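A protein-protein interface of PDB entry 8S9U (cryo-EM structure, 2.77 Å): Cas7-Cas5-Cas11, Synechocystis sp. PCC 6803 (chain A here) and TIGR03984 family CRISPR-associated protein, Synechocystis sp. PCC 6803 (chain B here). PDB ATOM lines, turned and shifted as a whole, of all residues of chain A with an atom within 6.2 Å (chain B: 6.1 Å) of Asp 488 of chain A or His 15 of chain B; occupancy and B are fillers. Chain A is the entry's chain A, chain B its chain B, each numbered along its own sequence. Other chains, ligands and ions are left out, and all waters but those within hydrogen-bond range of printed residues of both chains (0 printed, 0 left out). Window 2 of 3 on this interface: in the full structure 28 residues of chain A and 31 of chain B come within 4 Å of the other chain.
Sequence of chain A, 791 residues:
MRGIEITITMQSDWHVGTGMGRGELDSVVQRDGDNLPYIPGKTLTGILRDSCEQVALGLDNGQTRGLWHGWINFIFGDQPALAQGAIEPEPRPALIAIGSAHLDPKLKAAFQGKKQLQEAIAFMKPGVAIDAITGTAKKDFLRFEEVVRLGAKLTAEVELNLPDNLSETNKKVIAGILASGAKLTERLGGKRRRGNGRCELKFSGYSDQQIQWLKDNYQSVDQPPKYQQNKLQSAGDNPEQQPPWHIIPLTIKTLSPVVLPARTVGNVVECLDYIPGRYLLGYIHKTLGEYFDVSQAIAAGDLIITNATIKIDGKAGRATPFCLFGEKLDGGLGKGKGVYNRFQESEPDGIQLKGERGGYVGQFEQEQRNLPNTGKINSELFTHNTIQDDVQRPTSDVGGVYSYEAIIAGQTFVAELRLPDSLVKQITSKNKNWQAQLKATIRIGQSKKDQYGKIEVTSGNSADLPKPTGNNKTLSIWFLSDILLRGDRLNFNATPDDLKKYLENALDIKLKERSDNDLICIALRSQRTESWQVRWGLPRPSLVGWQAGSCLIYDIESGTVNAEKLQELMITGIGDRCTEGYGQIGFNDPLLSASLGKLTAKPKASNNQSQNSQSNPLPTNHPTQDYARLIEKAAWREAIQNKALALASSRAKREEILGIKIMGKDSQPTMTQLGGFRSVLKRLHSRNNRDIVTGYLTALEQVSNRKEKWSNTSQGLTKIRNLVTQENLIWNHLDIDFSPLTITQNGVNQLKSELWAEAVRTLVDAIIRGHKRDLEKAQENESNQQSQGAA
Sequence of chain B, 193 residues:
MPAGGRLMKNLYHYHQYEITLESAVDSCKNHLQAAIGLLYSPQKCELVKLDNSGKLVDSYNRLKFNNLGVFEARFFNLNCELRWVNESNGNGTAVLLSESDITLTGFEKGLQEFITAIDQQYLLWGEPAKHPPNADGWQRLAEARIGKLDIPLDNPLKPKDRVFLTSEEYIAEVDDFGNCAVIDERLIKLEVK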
ATOM      1  N   ARG A 486      32.189   8.261 -19.297  1.00  0.00           N
ATOM      2  CA  ARG A 486      30.833   8.774 -19.324  1.00  0.00           C
ATOM      3  C   ARG A 486      30.247   8.625 -20.717  1.00  0.00           C
ATOM      4  O   ARG A 486      30.943   8.802 -21.718  1.00  0.00           O
ATOM      5  CB  ARG A 486      30.796  10.237 -18.902  1.00  0.00           C
ATOM      6  CG  ARG A 486      31.196  10.443 -17.478  1.00  0.00           C
ATOM      7  CD  ARG A 486      31.309  11.895 -17.144  1.00  0.00           C
ATOM      8  NE  ARG A 486      31.783  12.078 -15.782  1.00  0.00           N
ATOM      9  CZ  ARG A 486      30.992  12.330 -14.750  1.00  0.00           C
ATOM     10  NH1 ARG A 486      29.681  12.337 -14.909  1.00  0.00           N
ATOM     11  NH2 ARG A 486      31.510  12.497 -13.545  1.00  0.00           N
ATOM     12  N   GLY A 487      28.963   8.311 -20.779  1.00  0.00           N
ATOM     13  CA  GLY A 487      28.254   8.378 -22.032  1.00  0.00           C
ATOM     14  C   GLY A 487      28.165   9.805 -22.522  1.00  0.00           C
ATOM     15  O   GLY A 487      28.622  10.754 -21.885  1.00  0.00           O
ATOM     16  N   ASP A 488      27.581   9.960 -23.709  1.00  0.00           N
ATOM     17  CA  ASP A 488      27.429  11.297 -24.265  1.00  0.00           C
ATOM     18  C   ASP A 488      26.495  12.169 -23.436  1.00  0.00           C
ATOM     19  O   ASP A 488      26.518  13.392 -23.587  1.00  0.00           O
ATOM     20  CB  ASP A 488      26.940  11.215 -25.709  1.00  0.00           C
ATOM     21  CG  ASP A 488      25.644  10.456 -25.841  1.00  0.00           C
ATOM     22  OD1 ASP A 488      25.313   9.679 -24.921  1.00  0.00           O
ATOM     23  OD2 ASP A 488      24.950  10.639 -26.864  1.00  0.00           O
ATOM     24  N   ARG A 489      25.693  11.577 -22.555  1.00  0.00           N
ATOM     25  CA  ARG A 489      24.863  12.318 -21.618  1.00  0.00           C
ATOM     26  C   ARG A 489      25.503  12.449 -20.246  1.00  0.00           C
ATOM     27  O   ARG A 489      24.794  12.672 -19.262  1.00  0.00           O
ATOM     28  CB  ARG A 489      23.495  11.665 -21.497  1.00  0.00           C
ATOM     29  CG  ARG A 489      22.816  11.493 -22.816  1.00  0.00           C
ATOM     30  CD  ARG A 489      21.508  10.785 -22.649  1.00  0.00           C
ATOM     31  NE  ARG A 489      20.997  10.379 -23.944  1.00  0.00           N
ATOM     32  CZ  ARG A 489      21.071   9.143 -24.413  1.00  0.00           C
ATOM     33  NH1 ARG A 489      21.398   8.144 -23.609  1.00  0.00           N
ATOM     34  NH2 ARG A 489      20.606   8.880 -25.621  1.00  0.00           N
ATOM     35  N   LEU A 490      26.818  12.274 -20.158  1.00  0.00           N
ATOM     36  CA  LEU A 490      27.589  12.512 -18.944  1.00  0.00           C
ATOM     37  C   LEU A 490      27.268  11.570 -17.792  1.00  0.00           C
ATOM     38  O   LEU A 490      27.958  11.602 -16.771  1.00  0.00           O
ATOM     39  CB  LEU A 490      27.411  13.963 -18.492  1.00  0.00           C
ATOM     40  CG  LEU A 490      27.771  15.005 -19.546  1.00  0.00           C
ATOM     41  CD1 LEU A 490      27.501  16.392 -19.050  1.00  0.00           C
ATOM     42  CD2 LEU A 490      29.206  14.860 -19.950  1.00  0.00           C
ATOM     43  N   ASN A 491      26.232  10.750 -17.913  1.00  0.00           N
ATOM     44  CA  ASN A 491      26.119   9.619 -17.006  1.00  0.00           C
ATOM     45  C   ASN A 491      27.106   8.528 -17.406  1.00  0.00           C
ATOM     46  O   ASN A 491      27.683   8.544 -18.493  1.00  0.00           O
ATOM     47  CB  ASN A 491      24.699   9.061 -16.997  1.00  0.00           C
ATOM     48  CG  ASN A 491      24.163   8.799 -18.388  1.00  0.00           C
ATOM     49  OD1 ASN A 491      24.857   8.986 -19.382  1.00  0.00           O
ATOM     50  ND2 ASN A 491      22.914   8.366 -18.462  1.00  0.00           N
ATOM     51  N   ASN A 493      26.738   5.430 -18.146  1.00  0.00           N
ATOM     52  CA  ASN A 493      26.255   4.298 -18.929  1.00  0.00           C
ATOM     53  C   ASN A 493      26.858   4.241 -20.328  1.00  0.00           C
ATOM     54  O   ASN A 493      26.161   3.978 -21.308  1.00  0.00           O
ATOM     55  CB  ASN A 493      24.729   4.340 -18.978  1.00  0.00           C
ATOM     56  CG  ASN A 493      24.197   5.488 -19.807  1.00  0.00           C
ATOM     57  OD1 ASN A 493      24.947   6.354 -20.252  1.00  0.00           O
ATOM     58  ND2 ASN A 493      22.889   5.505 -20.010  1.00  0.00           N
ATOM     59  N   ALA A 494      28.160   4.488 -20.440  1.00  0.00           N
ATOM     60  CA  ALA A 494      28.883   4.319 -21.687  1.00  0.00           C
ATOM     61  C   ALA A 494      28.922   2.851 -22.104  1.00  0.00           C
ATOM     62  O   ALA A 494      28.635   1.940 -21.323  1.00  0.00           O
ATOM     63  CB  ALA A 494      30.304   4.860 -21.559  1.00  0.00           C
ATOM     64  N   ASP A 498      31.470   3.734 -27.161  1.00  0.00           N
ATOM     65  CA  ASP A 498      32.004   4.962 -26.583  1.00  0.00           C
ATOM     66  C   ASP A 498      33.510   4.884 -26.380  1.00  0.00           C
ATOM     67  O   ASP A 498      34.216   5.879 -26.570  1.00  0.00           O
ATOM     68  CB  ASP A 498      31.313   5.264 -25.257  1.00  0.00           C
ATOM     69  CG  ASP A 498      29.819   5.397 -25.398  1.00  0.00           C
ATOM     70  OD1 ASP A 498      29.366   6.404 -25.976  1.00  0.00           O
ATOM     71  OD2 ASP A 498      29.093   4.497 -24.932  1.00  0.00           O
ATOM     72  N   HIS B  13      18.217  15.651 -26.013  1.00  0.00           N
ATOM     73  CA  HIS B  13      19.414  15.961 -25.246  1.00  0.00           C
ATOM     74  C   HIS B  13      20.291  16.916 -26.035  1.00  0.00           C
ATOM     75  O   HIS B  13      20.526  16.705 -27.227  1.00  0.00           O
ATOM     76  CB  HIS B  13      20.198  14.689 -24.927  1.00  0.00           C
ATOM     77  CG  HIS B  13      20.469  13.841 -26.127  1.00  0.00           C
ATOM     78  ND1 HIS B  13      21.440  14.152 -27.051  1.00  0.00           N
ATOM     79  CD2 HIS B  13      19.886  12.702 -26.565  1.00  0.00           C
ATOM     80  CE1 HIS B  13      21.449  13.238 -28.004  1.00  0.00           C
ATOM     81  NE2 HIS B  13      20.516  12.346 -27.731  1.00  0.00           N
ATOM     82  N   TYR B  14      20.762  17.966 -25.371  1.00  0.00           N
ATOM     83  CA  TYR B  14      21.430  19.078 -26.026  1.00  0.00           C
ATOM     84  C   TYR B  14      22.851  19.196 -25.501  1.00  0.00           C
ATOM     85  O   TYR B  14      23.053  19.305 -24.291  1.00  0.00           O
ATOM     86  CB  TYR B  14      20.663  20.370 -25.776  1.00  0.00           C
ATOM     87  CG  TYR B  14      19.227  20.288 -26.215  1.00  0.00           C
ATOM     88  CD1 TYR B  14      18.259  19.750 -25.381  1.00  0.00           C
ATOM     89  CD2 TYR B  14      18.838  20.723 -27.469  1.00  0.00           C
ATOM     90  CE1 TYR B  14      16.951  19.667 -25.772  1.00  0.00           C
ATOM     91  CE2 TYR B  14      17.530  20.641 -27.870  1.00  0.00           C
ATOM     92  CZ  TYR B  14      16.591  20.112 -27.018  1.00  0.00           C
ATOM     93  OH  TYR B  14      15.283  20.027 -27.422  1.00  0.00           O
ATOM     94  N   HIS B  15      23.830  19.188 -26.397  1.00  0.00           N
ATOM     95  CA  HIS B  15      25.231  19.216 -26.007  1.00  0.00           C
ATOM     96  C   HIS B  15      25.849  20.567 -26.326  1.00  0.00           C
ATOM     97  O   HIS B  15      25.594  21.140 -27.387  1.00  0.00           O
ATOM     98  CB  HIS B  15      26.031  18.123 -26.712  1.00  0.00           C
ATOM     99  CG  HIS B  15      25.434  16.760 -26.585  1.00  0.00           C
ATOM    100  ND1 HIS B  15      25.863  15.847 -25.649  1.00  0.00           N
ATOM    101  CD2 HIS B  15      24.446  16.151 -27.280  1.00  0.00           C
ATOM    102  CE1 HIS B  15      25.161  14.735 -25.769  1.00  0.00           C
ATOM    103  NE2 HIS B  15      24.294  14.895 -26.751  1.00  0.00           N
ATOM    104  N   GLN B  16      26.661  21.071 -25.401  1.00  0.00           N
ATOM    105  CA  GLN B  16      27.601  22.142 -25.683  1.00  0.00           C
ATOM    106  C   GLN B  16      28.927  21.825 -25.014  1.00  0.00           C
ATOM    107  O   GLN B  16      28.952  21.319 -23.891  1.00  0.00           O
ATOM    108  CB  GLN B  16      27.080  23.493 -25.196  1.00  0.00           C
ATOM    109  CG  GLN B  16      27.921  24.663 -25.645  1.00  0.00           C
ATOM    110  CD  GLN B  16      27.277  25.988 -25.334  1.00  0.00           C
ATOM    111  OE1 GLN B  16      26.386  26.073 -24.495  1.00  0.00           O
ATOM    112  NE2 GLN B  16      27.719  27.034 -26.016  1.00  0.00           N
ATOM    113  N   TYR B  17      30.023  22.131 -25.696  1.00  0.00           N
ATOM    114  CA  TYR B  17      31.354  21.751 -25.254  1.00  0.00           C
ATOM    115  C   TYR B  17      32.204  22.982 -24.970  1.00  0.00           C
ATOM    116  O   TYR B  17      31.952  24.076 -25.482  1.00  0.00           O
ATOM    117  CB  TYR B  17      32.062  20.854 -26.275  1.00  0.00           C
ATOM    118  CG  TYR B  17      31.174  19.816 -26.910  1.00  0.00           C
ATOM    119  CD1 TYR B  17      30.886  18.632 -26.249  1.00  0.00           C
ATOM    120  CD2 TYR B  17      30.618  20.020 -28.157  1.00  0.00           C
ATOM    121  CE1 TYR B  17      30.082  17.677 -26.820  1.00  0.00           C
ATOM    122  CE2 TYR B  17      29.806  19.073 -28.733  1.00  0.00           C
ATOM    123  CZ  TYR B  17      29.540  17.902 -28.060  1.00  0.00           C
ATOM    124  OH  TYR B  17      28.723  16.958 -28.637  1.00  0.00           O
ATOM    125  N   THR B  93      31.755  19.923 -20.592  1.00  0.00           N
ATOM    126  CA  THR B  93      30.609  19.613 -21.428  1.00  0.00           C
ATOM    127  C   THR B  93      29.325  19.848 -20.650  1.00  0.00           C
ATOM    128  O   THR B  93      29.206  19.425 -19.498  1.00  0.00           O
ATOM    129  CB  THR B  93      30.674  18.163 -21.904  1.00  0.00           C
ATOM    130  OG1 THR B  93      31.793  17.999 -22.780  1.00  0.00           O
ATOM    131  CG2 THR B  93      29.419  17.793 -22.660  1.00  0.00           C
ATOM    132  N   ALA B  94      28.367  20.512 -21.286  1.00  0.00           N
ATOM    133  CA  ALA B  94      27.003  20.599 -20.794  1.00  0.00           C
ATOM    134  C   ALA B  94      26.121  19.674 -21.614  1.00  0.00           C
ATOM    135  O   ALA B  94      26.232  19.626 -22.839  1.00  0.00           O
ATOM    136  CB  ALA B  94      26.478  22.030 -20.870  1.00  0.00           C
ATOM    137  N   VAL B  95      25.249  18.936 -20.937  1.00  0.00           N
ATOM    138  CA  VAL B  95      24.162  18.218 -21.586  1.00  0.00           C
ATOM    139  C   VAL B  95      22.880  18.550 -20.848  1.00  0.00           C
ATOM    140  O   VAL B  95      22.790  18.343 -19.635  1.00  0.00           O
ATOM    141  CB  VAL B  95      24.391  16.700 -21.604  1.00  0.00           C
ATOM    142  CG1 VAL B  95      23.265  16.011 -22.327  1.00  0.00           C
ATOM    143  CG2 VAL B  95      25.703  16.374 -22.275  1.00  0.00           C
ATOM    144  N   LEU B  96      21.894  19.059 -21.573  1.00  0.00           N
ATOM    145  CA  LEU B  96      20.562  19.270 -21.031  1.00  0.00           C
ATOM    146  C   LEU B  96      19.642  18.181 -21.555  1.00  0.00           C
ATOM    147  O   LEU B  96      19.625  17.909 -22.757  1.00  0.00           O
ATOM    148  CB  LEU B  96      20.034  20.652 -21.411  1.00  0.00           C
ATOM    149  CG  LEU B  96      18.704  21.068 -20.795  1.00  0.00           C
ATOM    150  CD1 LEU B  96      18.747  22.526 -20.461  1.00  0.00           C
ATOM    151  CD2 LEU B  96      17.569  20.805 -21.745  1.00  0.00           C
ATOM    152  N   GLY B 106      23.792  27.893 -29.090  1.00  0.00           N
ATOM    153  CA  GLY B 106      25.090  27.258 -28.985  1.00  0.00           C
ATOM    154  C   GLY B 106      25.041  25.770 -28.726  1.00  0.00           C
ATOM    155  O   GLY B 106      25.908  25.021 -29.185  1.00  0.00           O
ATOM    156  N   PHE B 107      24.023  25.326 -28.000  1.00  0.00           N
ATOM    157  CA  PHE B 107      23.818  23.903 -27.801  1.00  0.00           C
ATOM    158  C   PHE B 107      23.509  23.222 -29.126  1.00  0.00           C
ATOM    159  O   PHE B 107      22.877  23.799 -30.014  1.00  0.00           O
ATOM    160  CB  PHE B 107      22.690  23.690 -26.800  1.00  0.00           C
ATOM    161  CG  PHE B 107      23.132  23.818 -25.378  1.00  0.00           C
ATOM    162  CD1 PHE B 107      23.132  25.049 -24.757  1.00  0.00           C
ATOM    163  CD2 PHE B 107      23.556  22.720 -24.666  1.00  0.00           C
ATOM    164  CE1 PHE B 107      23.543  25.180 -23.454  1.00  0.00           C
ATOM    165  CE2 PHE B 107      23.962  22.847 -23.361  1.00  0.00           C
ATOM    166  CZ  PHE B 107      23.956  24.075 -22.755  1.00  0.00           C
ATOM    167  N   GLU B 108      23.962  21.981 -29.257  1.00  0.00           N
ATOM    168  CA  GLU B 108      23.595  21.133 -30.379  1.00  0.00           C
ATOM    169  C   GLU B 108      22.493  20.184 -29.941  1.00  0.00           C
ATOM    170  O   GLU B 108      22.607  19.534 -28.901  1.00  0.00           O
ATOM    171  CB  GLU B 108      24.805  20.350 -30.880  1.00  0.00           C
ATOM    172  CG  GLU B 108      24.473  19.322 -31.932  1.00  0.00           C
ATOM    173  CD  GLU B 108      25.682  18.527 -32.360  1.00  0.00           C
ATOM    174  OE1 GLU B 108      26.562  18.289 -31.508  1.00  0.00           O
ATOM    175  OE2 GLU B 108      25.747  18.129 -33.540  1.00  0.00           O
ATOM    176  N   LYS B 109      21.446  20.081 -30.750  1.00  0.00           N
ATOM    177  CA  LYS B 109      20.357  19.173 -30.440  1.00  0.00           C
ATOM    178  C   LYS B 109      20.688  17.757 -30.879  1.00  0.00           C
ATOM    179  O   LYS B 109      21.376  17.532 -31.878  1.00  0.00           O
ATOM    180  CB  LYS B 109      19.059  19.640 -31.095  1.00  0.00           C
ATOM    181  CG  LYS B 109      17.859  18.766 -30.782  1.00  0.00           C
ATOM    182  CD  LYS B 109      16.571  19.437 -31.194  1.00  0.00           C
ATOM    183  CE  LYS B 109      16.449  19.533 -32.704  1.00  0.00           C
ATOM    184  NZ  LYS B 109      15.264  20.341 -33.095  1.00  0.00           N
ATOM    185  N   GLY B 110      20.193  16.797 -30.104  1.00  0.00           N
ATOM    186  CA  GLY B 110      20.053  15.425 -30.533  1.00  0.00           C
ATOM    187  C   GLY B 110      18.847  14.835 -29.841  1.00  0.00           C
ATOM    188  O   GLY B 110      18.145  15.516 -29.093  1.00  0.00           O
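Asp 488 of chain A touches Val 95 of chain B.
His 13 of chain B touches Arg 489 of chain A.
Thr 93 of chain B touches Leu 490 of chain A.
Val 95 of chain B touches Leu 490 of chain A (CG2 to CG, 3.7 Å).
The guanidinium group (NH1) of Arg 486 of chain A is in hydrogen-bond range of the backbone carbonyl oxygen (O) of Leu 490 of chain A (2.6 Å).
A ring nitrogen (ND1) of His 13 of chain B sits at hydrogen-bond distance from a ring nitrogen (NE2) of His 15 of chain B.
The backbone carbonyl oxygen of His 13 of chain B sits at hydrogen-bond distance from the backbone NH of Gly 110 of chain B.
O of His 15 of chain B sits at hydrogen-bond distance from N of Glu 108 of chain B, at 2.6 Å.
A ring nitrogen (ND1) of His 15 of chain B sits close to the backbone carbonyl oxygen (O) of Asp 488 of chain A.
Of the 9 printed residues of chain A, 3 touch a printed residue of chain B.
Hydrophobic or aromatic side chains of chain A that line the printed part of chain B: Leu 490.
Along chain A the printed residues that touch a printed residue of chain B span positions 488 to 490.
Of the 14 printed residues of chain B, 4 touch a printed residue of chain A.
Among the printed residues, 5 pairs touch across the chains.
Among the printed residues, no Asp or Glu carboxylate lies within 4 Å of a Lys or Arg side-chain nitrogen of the other chain.
Of chain B, only His 15 and Val 95 come within 4 Å of Asp 488 of chain A.
Of the printed residues of chain A, His 15 of chain B touches Asp 488.
Of the printed residues of chain B, Leu 490 of chain A touches Thr 93 and Val 95.
Printed residues of chain A within 4 Å of Thr 93 of chain B: Leu 490 (3.5 Å).
Of the printed residues of chain A, Val 95 of chain B touches Asp 488 and Leu 490.
Of the printed residues of chain A, His 13 of chain B touches Arg 489 (3.7 Å).
Gly 106 of chain B touches none of the printed residues of chain A.
The nearest residue of chain A that does not touch His 15 of chain B is Arg 489 of chain A (4.5 Å).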
